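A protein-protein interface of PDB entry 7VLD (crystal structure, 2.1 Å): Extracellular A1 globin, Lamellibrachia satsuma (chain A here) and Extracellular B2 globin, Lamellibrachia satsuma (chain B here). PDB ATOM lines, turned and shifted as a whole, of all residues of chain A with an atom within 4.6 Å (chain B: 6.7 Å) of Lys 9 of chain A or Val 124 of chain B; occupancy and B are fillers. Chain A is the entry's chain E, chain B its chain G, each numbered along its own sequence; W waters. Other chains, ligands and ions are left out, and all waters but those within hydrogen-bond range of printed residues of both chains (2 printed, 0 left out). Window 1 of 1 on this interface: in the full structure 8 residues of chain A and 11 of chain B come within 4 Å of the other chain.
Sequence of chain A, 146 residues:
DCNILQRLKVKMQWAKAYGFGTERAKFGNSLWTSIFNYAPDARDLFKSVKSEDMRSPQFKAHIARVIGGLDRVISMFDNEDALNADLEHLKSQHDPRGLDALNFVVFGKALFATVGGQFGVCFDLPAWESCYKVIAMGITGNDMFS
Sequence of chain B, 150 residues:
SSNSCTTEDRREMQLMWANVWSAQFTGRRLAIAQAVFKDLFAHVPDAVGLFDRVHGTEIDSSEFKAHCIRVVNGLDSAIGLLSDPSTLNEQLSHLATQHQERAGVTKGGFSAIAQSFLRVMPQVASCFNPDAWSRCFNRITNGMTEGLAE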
ATOM      1  N   LEU A   5      17.078 -10.960  16.750  1.00  0.00           N
ATOM      2  CA  LEU A   5      17.889 -11.147  15.552  1.00  0.00           C
ATOM      3  C   LEU A   5      18.258 -12.613  15.359  1.00  0.00           C
ATOM      4  O   LEU A   5      18.242 -13.119  14.231  1.00  0.00           O
ATOM      5  CB  LEU A   5      19.142 -10.275  15.620  1.00  0.00           C
ATOM      6  CG  LEU A   5      18.901  -8.765  15.555  1.00  0.00           C
ATOM      7  CD1 LEU A   5      20.221  -8.011  15.526  1.00  0.00           C
ATOM      8  CD2 LEU A   5      18.046  -8.409  14.347  1.00  0.00           C
ATOM      9  N   GLN A   6      18.588 -13.313  16.449  1.00  0.00           N
ATOM     10  CA  GLN A   6      18.862 -14.743  16.349  1.00  0.00           C
ATOM     11  C   GLN A   6      17.618 -15.510  15.912  1.00  0.00           C
ATOM     12  O   GLN A   6      17.715 -16.481  15.152  1.00  0.00           O
ATOM     13  CB  GLN A   6      19.383 -15.277  17.685  1.00  0.00           C
ATOM     14  CG  GLN A   6      20.804 -14.844  18.027  1.00  0.00           C
ATOM     15  CD  GLN A   6      21.264 -15.354  19.382  1.00  0.00           C
ATOM     16  OE1 GLN A   6      20.634 -15.085  20.405  1.00  0.00           O
ATOM     17  NE2 GLN A   6      22.365 -16.096  19.397  1.00  0.00           N
ATOM     18  N   ARG A   7      16.439 -15.086  16.378  1.00  0.00           N
ATOM     19  CA  ARG A   7      15.201 -15.748  15.976  1.00  0.00           C
ATOM     20  C   ARG A   7      14.950 -15.590  14.482  1.00  0.00           C
ATOM     21  O   ARG A   7      14.511 -16.535  13.816  1.00  0.00           O
ATOM     22  CB  ARG A   7      14.025 -15.200  16.786  1.00  0.00           C
ATOM     23  CG  ARG A   7      14.038 -15.626  18.244  1.00  0.00           C
ATOM     24  CD  ARG A   7      13.071 -14.828  19.106  1.00  0.00           C
ATOM     25  NE  ARG A   7      13.356 -15.012  20.529  1.00  0.00           N
ATOM     26  CZ  ARG A   7      12.621 -15.748  21.357  1.00  0.00           C
ATOM     27  NH1 ARG A   7      11.536 -16.368  20.917  1.00  0.00           N
ATOM     28  NH2 ARG A   7      12.968 -15.855  22.633  1.00  0.00           N
ATOM     29  N   LEU A   8      15.226 -14.403  13.936  1.00  0.00           N
ATOM     30  CA  LEU A   8      15.063 -14.194  12.501  1.00  0.00           C
ATOM     31  C   LEU A   8      16.030 -15.058  11.704  1.00  0.00           C
ATOM     32  O   LEU A   8      15.661 -15.628  10.671  1.00  0.00           O
ATOM     33  CB  LEU A   8      15.262 -12.719  12.156  1.00  0.00           C
ATOM     34  CG  LEU A   8      14.208 -11.740  12.672  1.00  0.00           C
ATOM     35  CD1 LEU A   8      14.530 -10.339  12.193  1.00  0.00           C
ATOM     36  CD2 LEU A   8      12.818 -12.159  12.221  1.00  0.00           C
ATOM     37  N   LYS A   9      17.278 -15.163  12.167  1.00  0.00           N
ATOM     38  CA  LYS A   9      18.265 -15.983  11.474  1.00  0.00           C
ATOM     39  C   LYS A   9      17.842 -17.447  11.445  1.00  0.00           C
ATOM     40  O   LYS A   9      17.934 -18.109  10.405  1.00  0.00           O
ATOM     41  CB  LYS A   9      19.628 -15.824  12.149  1.00  0.00           C
ATOM     42  CG  LYS A   9      20.764 -16.605  11.509  1.00  0.00           C
ATOM     43  CD  LYS A   9      21.301 -15.901  10.277  1.00  0.00           C
ATOM     44  CE  LYS A   9      22.809 -16.062  10.169  1.00  0.00           C
ATOM     45  NZ  LYS A   9      23.525 -15.357  11.271  1.00  0.00           N
ATOM     46  N   VAL A  10      17.355 -17.963  12.577  1.00  0.00           N
ATOM     47  CA  VAL A  10      16.972 -19.370  12.660  1.00  0.00           C
ATOM     48  C   VAL A  10      15.782 -19.663  11.752  1.00  0.00           C
ATOM     49  O   VAL A  10      15.746 -20.696  11.071  1.00  0.00           O
ATOM     50  CB  VAL A  10      16.685 -19.754  14.124  1.00  0.00           C
ATOM     51  CG1 VAL A  10      15.956 -21.086  14.200  1.00  0.00           C
ATOM     52  CG2 VAL A  10      17.985 -19.814  14.918  1.00  0.00           C
ATOM     53  N   LYS A  11      14.790 -18.768  11.725  1.00  0.00           N
ATOM     54  CA  LYS A  11      13.655 -18.947  10.821  1.00  0.00           C
ATOM     55  C   LYS A  11      14.114 -18.998   9.369  1.00  0.00           C
ATOM     56  O   LYS A  11      13.662 -19.849   8.594  1.00  0.00           O
ATOM     57  CB  LYS A  11      12.643 -17.820  11.017  1.00  0.00           C
ATOM     58  CG  LYS A  11      11.963 -17.815  12.374  1.00  0.00           C
ATOM     59  CD  LYS A  11      11.350 -16.455  12.676  1.00  0.00           C
ATOM     60  CE  LYS A  11      10.361 -16.039  11.602  1.00  0.00           C
ATOM     61  NZ  LYS A  11       9.196 -16.963  11.534  1.00  0.00           N
ATOM     62  N   MET A  12      15.014 -18.089   8.991  1.00  0.00           N
ATOM     63  CA  MET A  12      15.565 -18.065   7.640  1.00  0.00           C
ATOM     64  C   MET A  12      16.216 -19.397   7.288  1.00  0.00           C
ATOM     65  O   MET A  12      15.863 -20.039   6.291  1.00  0.00           O
ATOM     66  CB  MET A  12      16.586 -16.931   7.531  1.00  0.00           C
ATOM     67  CG  MET A  12      16.561 -16.158   6.233  1.00  0.00           C
ATOM     68  SD  MET A  12      15.656 -14.614   6.411  1.00  0.00           S
ATOM     69  CE  MET A  12      14.250 -14.969   5.369  1.00  0.00           C
ATOM     70  N   GLN A  13      17.178 -19.828   8.109  1.00  0.00           N
ATOM     71  CA  GLN A  13      17.938 -21.033   7.800  1.00  0.00           C
ATOM     72  C   GLN A  13      17.072 -22.285   7.874  1.00  0.00           C
ATOM     73  O   GLN A  13      17.321 -23.248   7.142  1.00  0.00           O
ATOM     74  CB  GLN A  13      19.138 -21.144   8.742  1.00  0.00           C
ATOM     75  CG  GLN A  13      20.112 -19.979   8.612  1.00  0.00           C
ATOM     76  CD  GLN A  13      21.364 -20.151   9.453  1.00  0.00           C
ATOM     77  OE1 GLN A  13      21.414 -20.989  10.354  1.00  0.00           O
ATOM     78  NE2 GLN A  13      22.384 -19.355   9.157  1.00  0.00           N
ATOM     79  N   ASP A 124      24.376 -20.995  11.371  1.00  0.00           N
ATOM     80  CA  ASP A 124      24.723 -20.245  12.578  1.00  0.00           C
ATOM     81  C   ASP A 124      24.493 -21.159  13.777  1.00  0.00           C
ATOM     82  O   ASP A 124      23.420 -21.168  14.380  1.00  0.00           O
ATOM     83  CB  ASP A 124      23.902 -18.962  12.675  1.00  0.00           C
ATOM     84  CG  ASP A 124      24.504 -17.948  13.633  1.00  0.00           C
ATOM     85  OD1 ASP A 124      25.085 -18.356  14.662  1.00  0.00           O
ATOM     86  OD2 ASP A 124      24.396 -16.734  13.357  1.00  0.00           O
ATOM     87  N   ASN B  19      19.129 -12.085   0.858  1.00  0.00           N
ATOM     88  CA  ASN B  19      18.926 -13.249   1.714  1.00  0.00           C
ATOM     89  C   ASN B  19      18.251 -12.900   3.033  1.00  0.00           C
ATOM     90  O   ASN B  19      17.910 -13.812   3.795  1.00  0.00           O
ATOM     91  CB  ASN B  19      20.267 -13.932   1.996  1.00  0.00           C
ATOM     92  CG  ASN B  19      20.962 -14.403   0.733  1.00  0.00           C
ATOM     93  OD1 ASN B  19      20.479 -14.183  -0.377  1.00  0.00           O
ATOM     94  ND2 ASN B  19      22.111 -15.049   0.899  1.00  0.00           N
ATOM     95  N   VAL B  20      18.050 -11.612   3.319  1.00  0.00           N
ATOM     96  CA  VAL B  20      17.496 -11.160   4.585  1.00  0.00           C
ATOM     97  C   VAL B  20      16.224 -10.344   4.389  1.00  0.00           C
ATOM     98  O   VAL B  20      15.293 -10.435   5.196  1.00  0.00           O
ATOM     99  CB  VAL B  20      18.541 -10.346   5.376  1.00  0.00           C
ATOM    100  CG1 VAL B  20      18.035 -10.045   6.760  1.00  0.00           C
ATOM    101  CG2 VAL B  20      19.854 -11.100   5.442  1.00  0.00           C
ATOM    102  N   ARG B  28      10.546  -8.473   9.481  1.00  0.00           N
ATOM    103  CA  ARG B  28      11.993  -8.620   9.386  1.00  0.00           C
ATOM    104  C   ARG B  28      12.670  -7.285   9.098  1.00  0.00           C
ATOM    105  O   ARG B  28      13.740  -7.002   9.647  1.00  0.00           O
ATOM    106  CB  ARG B  28      12.346  -9.648   8.313  1.00  0.00           C
ATOM    107  CG  ARG B  28      13.820 -10.008   8.265  1.00  0.00           C
ATOM    108  CD  ARG B  28      14.023 -11.487   7.956  1.00  0.00           C
ATOM    109  NE  ARG B  28      13.425 -11.886   6.685  1.00  0.00           N
ATOM    110  CZ  ARG B  28      12.278 -12.551   6.572  1.00  0.00           C
ATOM    111  NH1 ARG B  28      11.812 -12.878   5.375  1.00  0.00           N
ATOM    112  NH2 ARG B  28      11.602 -12.899   7.657  1.00  0.00           N
ATOM    113  N   ILE B  32      15.365  -5.404  11.940  1.00  0.00           N
ATOM    114  CA  ILE B  32      16.715  -5.005  11.555  1.00  0.00           C
ATOM    115  C   ILE B  32      16.916  -3.513  11.785  1.00  0.00           C
ATOM    116  O   ILE B  32      17.964  -3.082  12.283  1.00  0.00           O
ATOM    117  CB  ILE B  32      16.987  -5.390  10.090  1.00  0.00           C
ATOM    118  CG1 ILE B  32      16.913  -6.905   9.912  1.00  0.00           C
ATOM    119  CG2 ILE B  32      18.341  -4.858   9.633  1.00  0.00           C
ATOM    120  CD1 ILE B  32      16.719  -7.323   8.483  1.00  0.00           C
ATOM    121  N   VAL B 120      25.084  -5.361  13.559  1.00  0.00           N
ATOM    122  CA  VAL B 120      23.762  -5.971  13.455  1.00  0.00           C
ATOM    123  C   VAL B 120      23.738  -7.051  12.379  1.00  0.00           C
ATOM    124  O   VAL B 120      23.254  -8.165  12.612  1.00  0.00           O
ATOM    125  CB  VAL B 120      22.701  -4.888  13.186  1.00  0.00           C
ATOM    126  CG1 VAL B 120      21.390  -5.522  12.743  1.00  0.00           C
ATOM    127  CG2 VAL B 120      22.489  -4.030  14.424  1.00  0.00           C
ATOM    128  N   MET B 121      24.260  -6.740  11.192  1.00  0.00           N
ATOM    129  CA  MET B 121      24.076  -7.623  10.041  1.00  0.00           C
ATOM    130  C   MET B 121      24.603  -9.044  10.234  1.00  0.00           C
ATOM    131  O   MET B 121      23.918  -9.983   9.790  1.00  0.00           O
ATOM    132  CB  MET B 121      24.703  -6.979   8.798  1.00  0.00           C
ATOM    133  CG  MET B 121      23.981  -5.732   8.307  1.00  0.00           C
ATOM    134  SD  MET B 121      22.273  -6.038   7.810  1.00  0.00           S
ATOM    135  CE  MET B 121      22.519  -7.151   6.431  1.00  0.00           C
ATOM    136  N   PRO B 122      25.769  -9.290  10.847  1.00  0.00           N
ATOM    137  CA  PRO B 122      26.186 -10.687  11.061  1.00  0.00           C
ATOM    138  C   PRO B 122      25.241 -11.482  11.947  1.00  0.00           C
ATOM    139  O   PRO B 122      25.271 -12.718  11.904  1.00  0.00           O
ATOM    140  CB  PRO B 122      27.576 -10.550  11.704  1.00  0.00           C
ATOM    141  CG  PRO B 122      27.625  -9.156  12.228  1.00  0.00           C
ATOM    142  CD  PRO B 122      26.827  -8.350  11.256  1.00  0.00           C
ATOM    143  N   GLN B 123      24.401 -10.820  12.744  1.00  0.00           N
ATOM    144  CA  GLN B 123      23.448 -11.532  13.586  1.00  0.00           C
ATOM    145  C   GLN B 123      22.211 -11.985  12.825  1.00  0.00           C
ATOM    146  O   GLN B 123      21.477 -12.846  13.320  1.00  0.00           O
ATOM    147  CB  GLN B 123      23.018 -10.651  14.762  1.00  0.00           C
ATOM    148  CG  GLN B 123      24.158 -10.159  15.632  1.00  0.00           C
ATOM    149  CD  GLN B 123      23.692  -9.179  16.691  1.00  0.00           C
ATOM    150  OE1 GLN B 123      22.813  -9.486  17.495  1.00  0.00           O
ATOM    151  NE2 GLN B 123      24.275  -7.985  16.688  1.00  0.00           N
ATOM    152  N   VAL B 124      21.960 -11.434  11.639  1.00  0.00           N
ATOM    153  CA  VAL B 124      20.720 -11.716  10.929  1.00  0.00           C
ATOM    154  C   VAL B 124      21.024 -12.289   9.548  1.00  0.00           C
ATOM    155  O   VAL B 124      20.263 -13.111   9.025  1.00  0.00           O
ATOM    156  CB  VAL B 124      19.846 -10.448  10.841  1.00  0.00           C
ATOM    157  CG1 VAL B 124      20.568  -9.333  10.092  1.00  0.00           C
ATOM    158  CG2 VAL B 124      18.498 -10.760  10.210  1.00  0.00           C
ATOM    159  N   ALA B 125      22.147 -11.884   8.962  1.00  0.00           N
ATOM    160  CA  ALA B 125      22.493 -12.286   7.606  1.00  0.00           C
ATOM    161  C   ALA B 125      23.393 -13.513   7.612  1.00  0.00           C
ATOM    162  O   ALA B 125      24.260 -13.662   8.479  1.00  0.00           O
ATOM    163  CB  ALA B 125      23.185 -11.141   6.865  1.00  0.00           C
ATOM    164  N   SER B 126      23.183 -14.389   6.633  1.00  0.00           N
ATOM    165  CA  SER B 126      24.039 -15.550   6.435  1.00  0.00           C
ATOM    166  C   SER B 126      25.155 -15.207   5.458  1.00  0.00           C
ATOM    167  O   SER B 126      24.952 -14.443   4.510  1.00  0.00           O
ATOM    168  CB  SER B 126      23.230 -16.739   5.911  1.00  0.00           C
ATOM    169  OG  SER B 126      22.251 -17.148   6.851  1.00  0.00           O
ATOM    170  N   CYS B 127      26.336 -15.778   5.701  1.00  0.00           N
ATOM    171  CA  CYS B 127      27.519 -15.549   4.867  1.00  0.00           C
ATOM    172  C   CYS B 127      27.851 -14.062   4.765  1.00  0.00           C
ATOM    173  O   CYS B 127      28.162 -13.554   3.686  1.00  0.00           O
ATOM    174  CB  CYS B 127      27.350 -16.143   3.465  1.00  0.00           C
ATOM    175  SG  CYS B 127      26.428 -17.692   3.319  1.00  0.00           S
HETATM  176  O   HOH W   1      23.104 -14.808  15.308  1.00  0.00           O
HETATM  177  O   HOH W   2      27.045 -15.016  12.872  1.00  0.00           O
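The backbone carbonyl oxygen of Leu 5 of chain A lies close to the backbone carbonyl oxygen of Gln 123 of chain B.
The side-chain hydroxyl of Ser 126 of chain B is in hydrogen-bond range of the side-chain amide nitrogen of Gln 13 of chain A, at 3.2 Å.
The side-chain amino group (NZ) of Lys 9 of chain A is in hydrogen-bond range of the backbone carbonyl oxygen (O) of Pro 122 of chain B.
NE of Arg 28 of chain B lies close to SD of Met 12 of chain A (3.5 Å).
O of Asn 19 of chain B lies close to SD of Met 12 of chain A (3.5 Å).
NZ of Lys 9 of chain A sits close to O of Ala 125 of chain B, 3.3 Å away.
The backbone NH (N) of Asp 124 of chain A is in hydrogen-bond range of the side-chain amide oxygen (OE1) of Gln 13 of chain A, at 3.1 Å.
The side-chain carboxylate (OD2) of Asp 124 of chain A is in salt-bridge range of the side-chain amino group (NZ) of Lys 9 of chain A (2.6 Å).
O of Val 20 of chain B lies within hydrogen-bond range of NE of Arg 28 of chain B (2.8 Å).
Among the printed residues, merely in contact across the chains: Lys 9 of chain A with Val 124 of chain B, Lys 9 of chain A with Ser 126 of chain B, Lys 9 of chain A with Gln 123 of chain B and Leu 5 of chain A with Val 120 of chain B.
Arg 7 of chain A touches none of the printed residues of chain B.
Of chain B, only Pro 122 (3.2 Å), Gln 123 (3.7 Å), Val 124 (3.2 Å), Ala 125 (3.3 Å) and Ser 126 (3.5 Å) come within 4 Å of Lys 9 of chain A.
Lys 11 of chain A touches none of the printed residues of chain B.
Of the printed residues of chain B, Gln 13 of chain A touches Ser 126.
Printed residues of chain A within 4 Å of Val 120 of chain B: Leu 5.
Val 124 of chain B touches just one residue of chain A: Lys 9.
Of the printed residues of chain A, Ala 125 of chain B touches Lys 9.
Printed residues of chain B that touch a printed residue of chain A: Asn 19, Arg 28, Val 120, Pro 122, Gln 123, Val 124, Ala 125 and Ser 126.
Of the 10 printed residues of chain A, 4 touch a printed residue of chain B.
Printed residues of chain A that touch a printed residue of chain B: Leu 5, Lys 9, Met 12 and Gln 13.
Hydrophobic or aromatic side chains of chain A within 4 Å of the printed part of chain B: Leu 5 and Met 12.
Along chain A the printed residues that touch a printed residue of chain B span positions 5 to 13.
Among the printed residues, 10 pairs touch across the chains.
Among the printed residues, no Asp or Glu carboxylate lies within 4 Å of a Lys or Arg side-chain nitrogen of the other chain.
Water W1 lies within hydrogen-bond range of the side-chain carboxylate (OD2) of Asp 124 of chain A (3.0 Å) and the backbone carbonyl oxygen (O) of Gln 123 of chain B (3.2 Å).
Water W2 bridges the backbone carbonyl oxygen of Pro 122 of chain B (3.1 Å) and the side-chain carboxylate of Asp 124 of chain A (3.2 Å).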
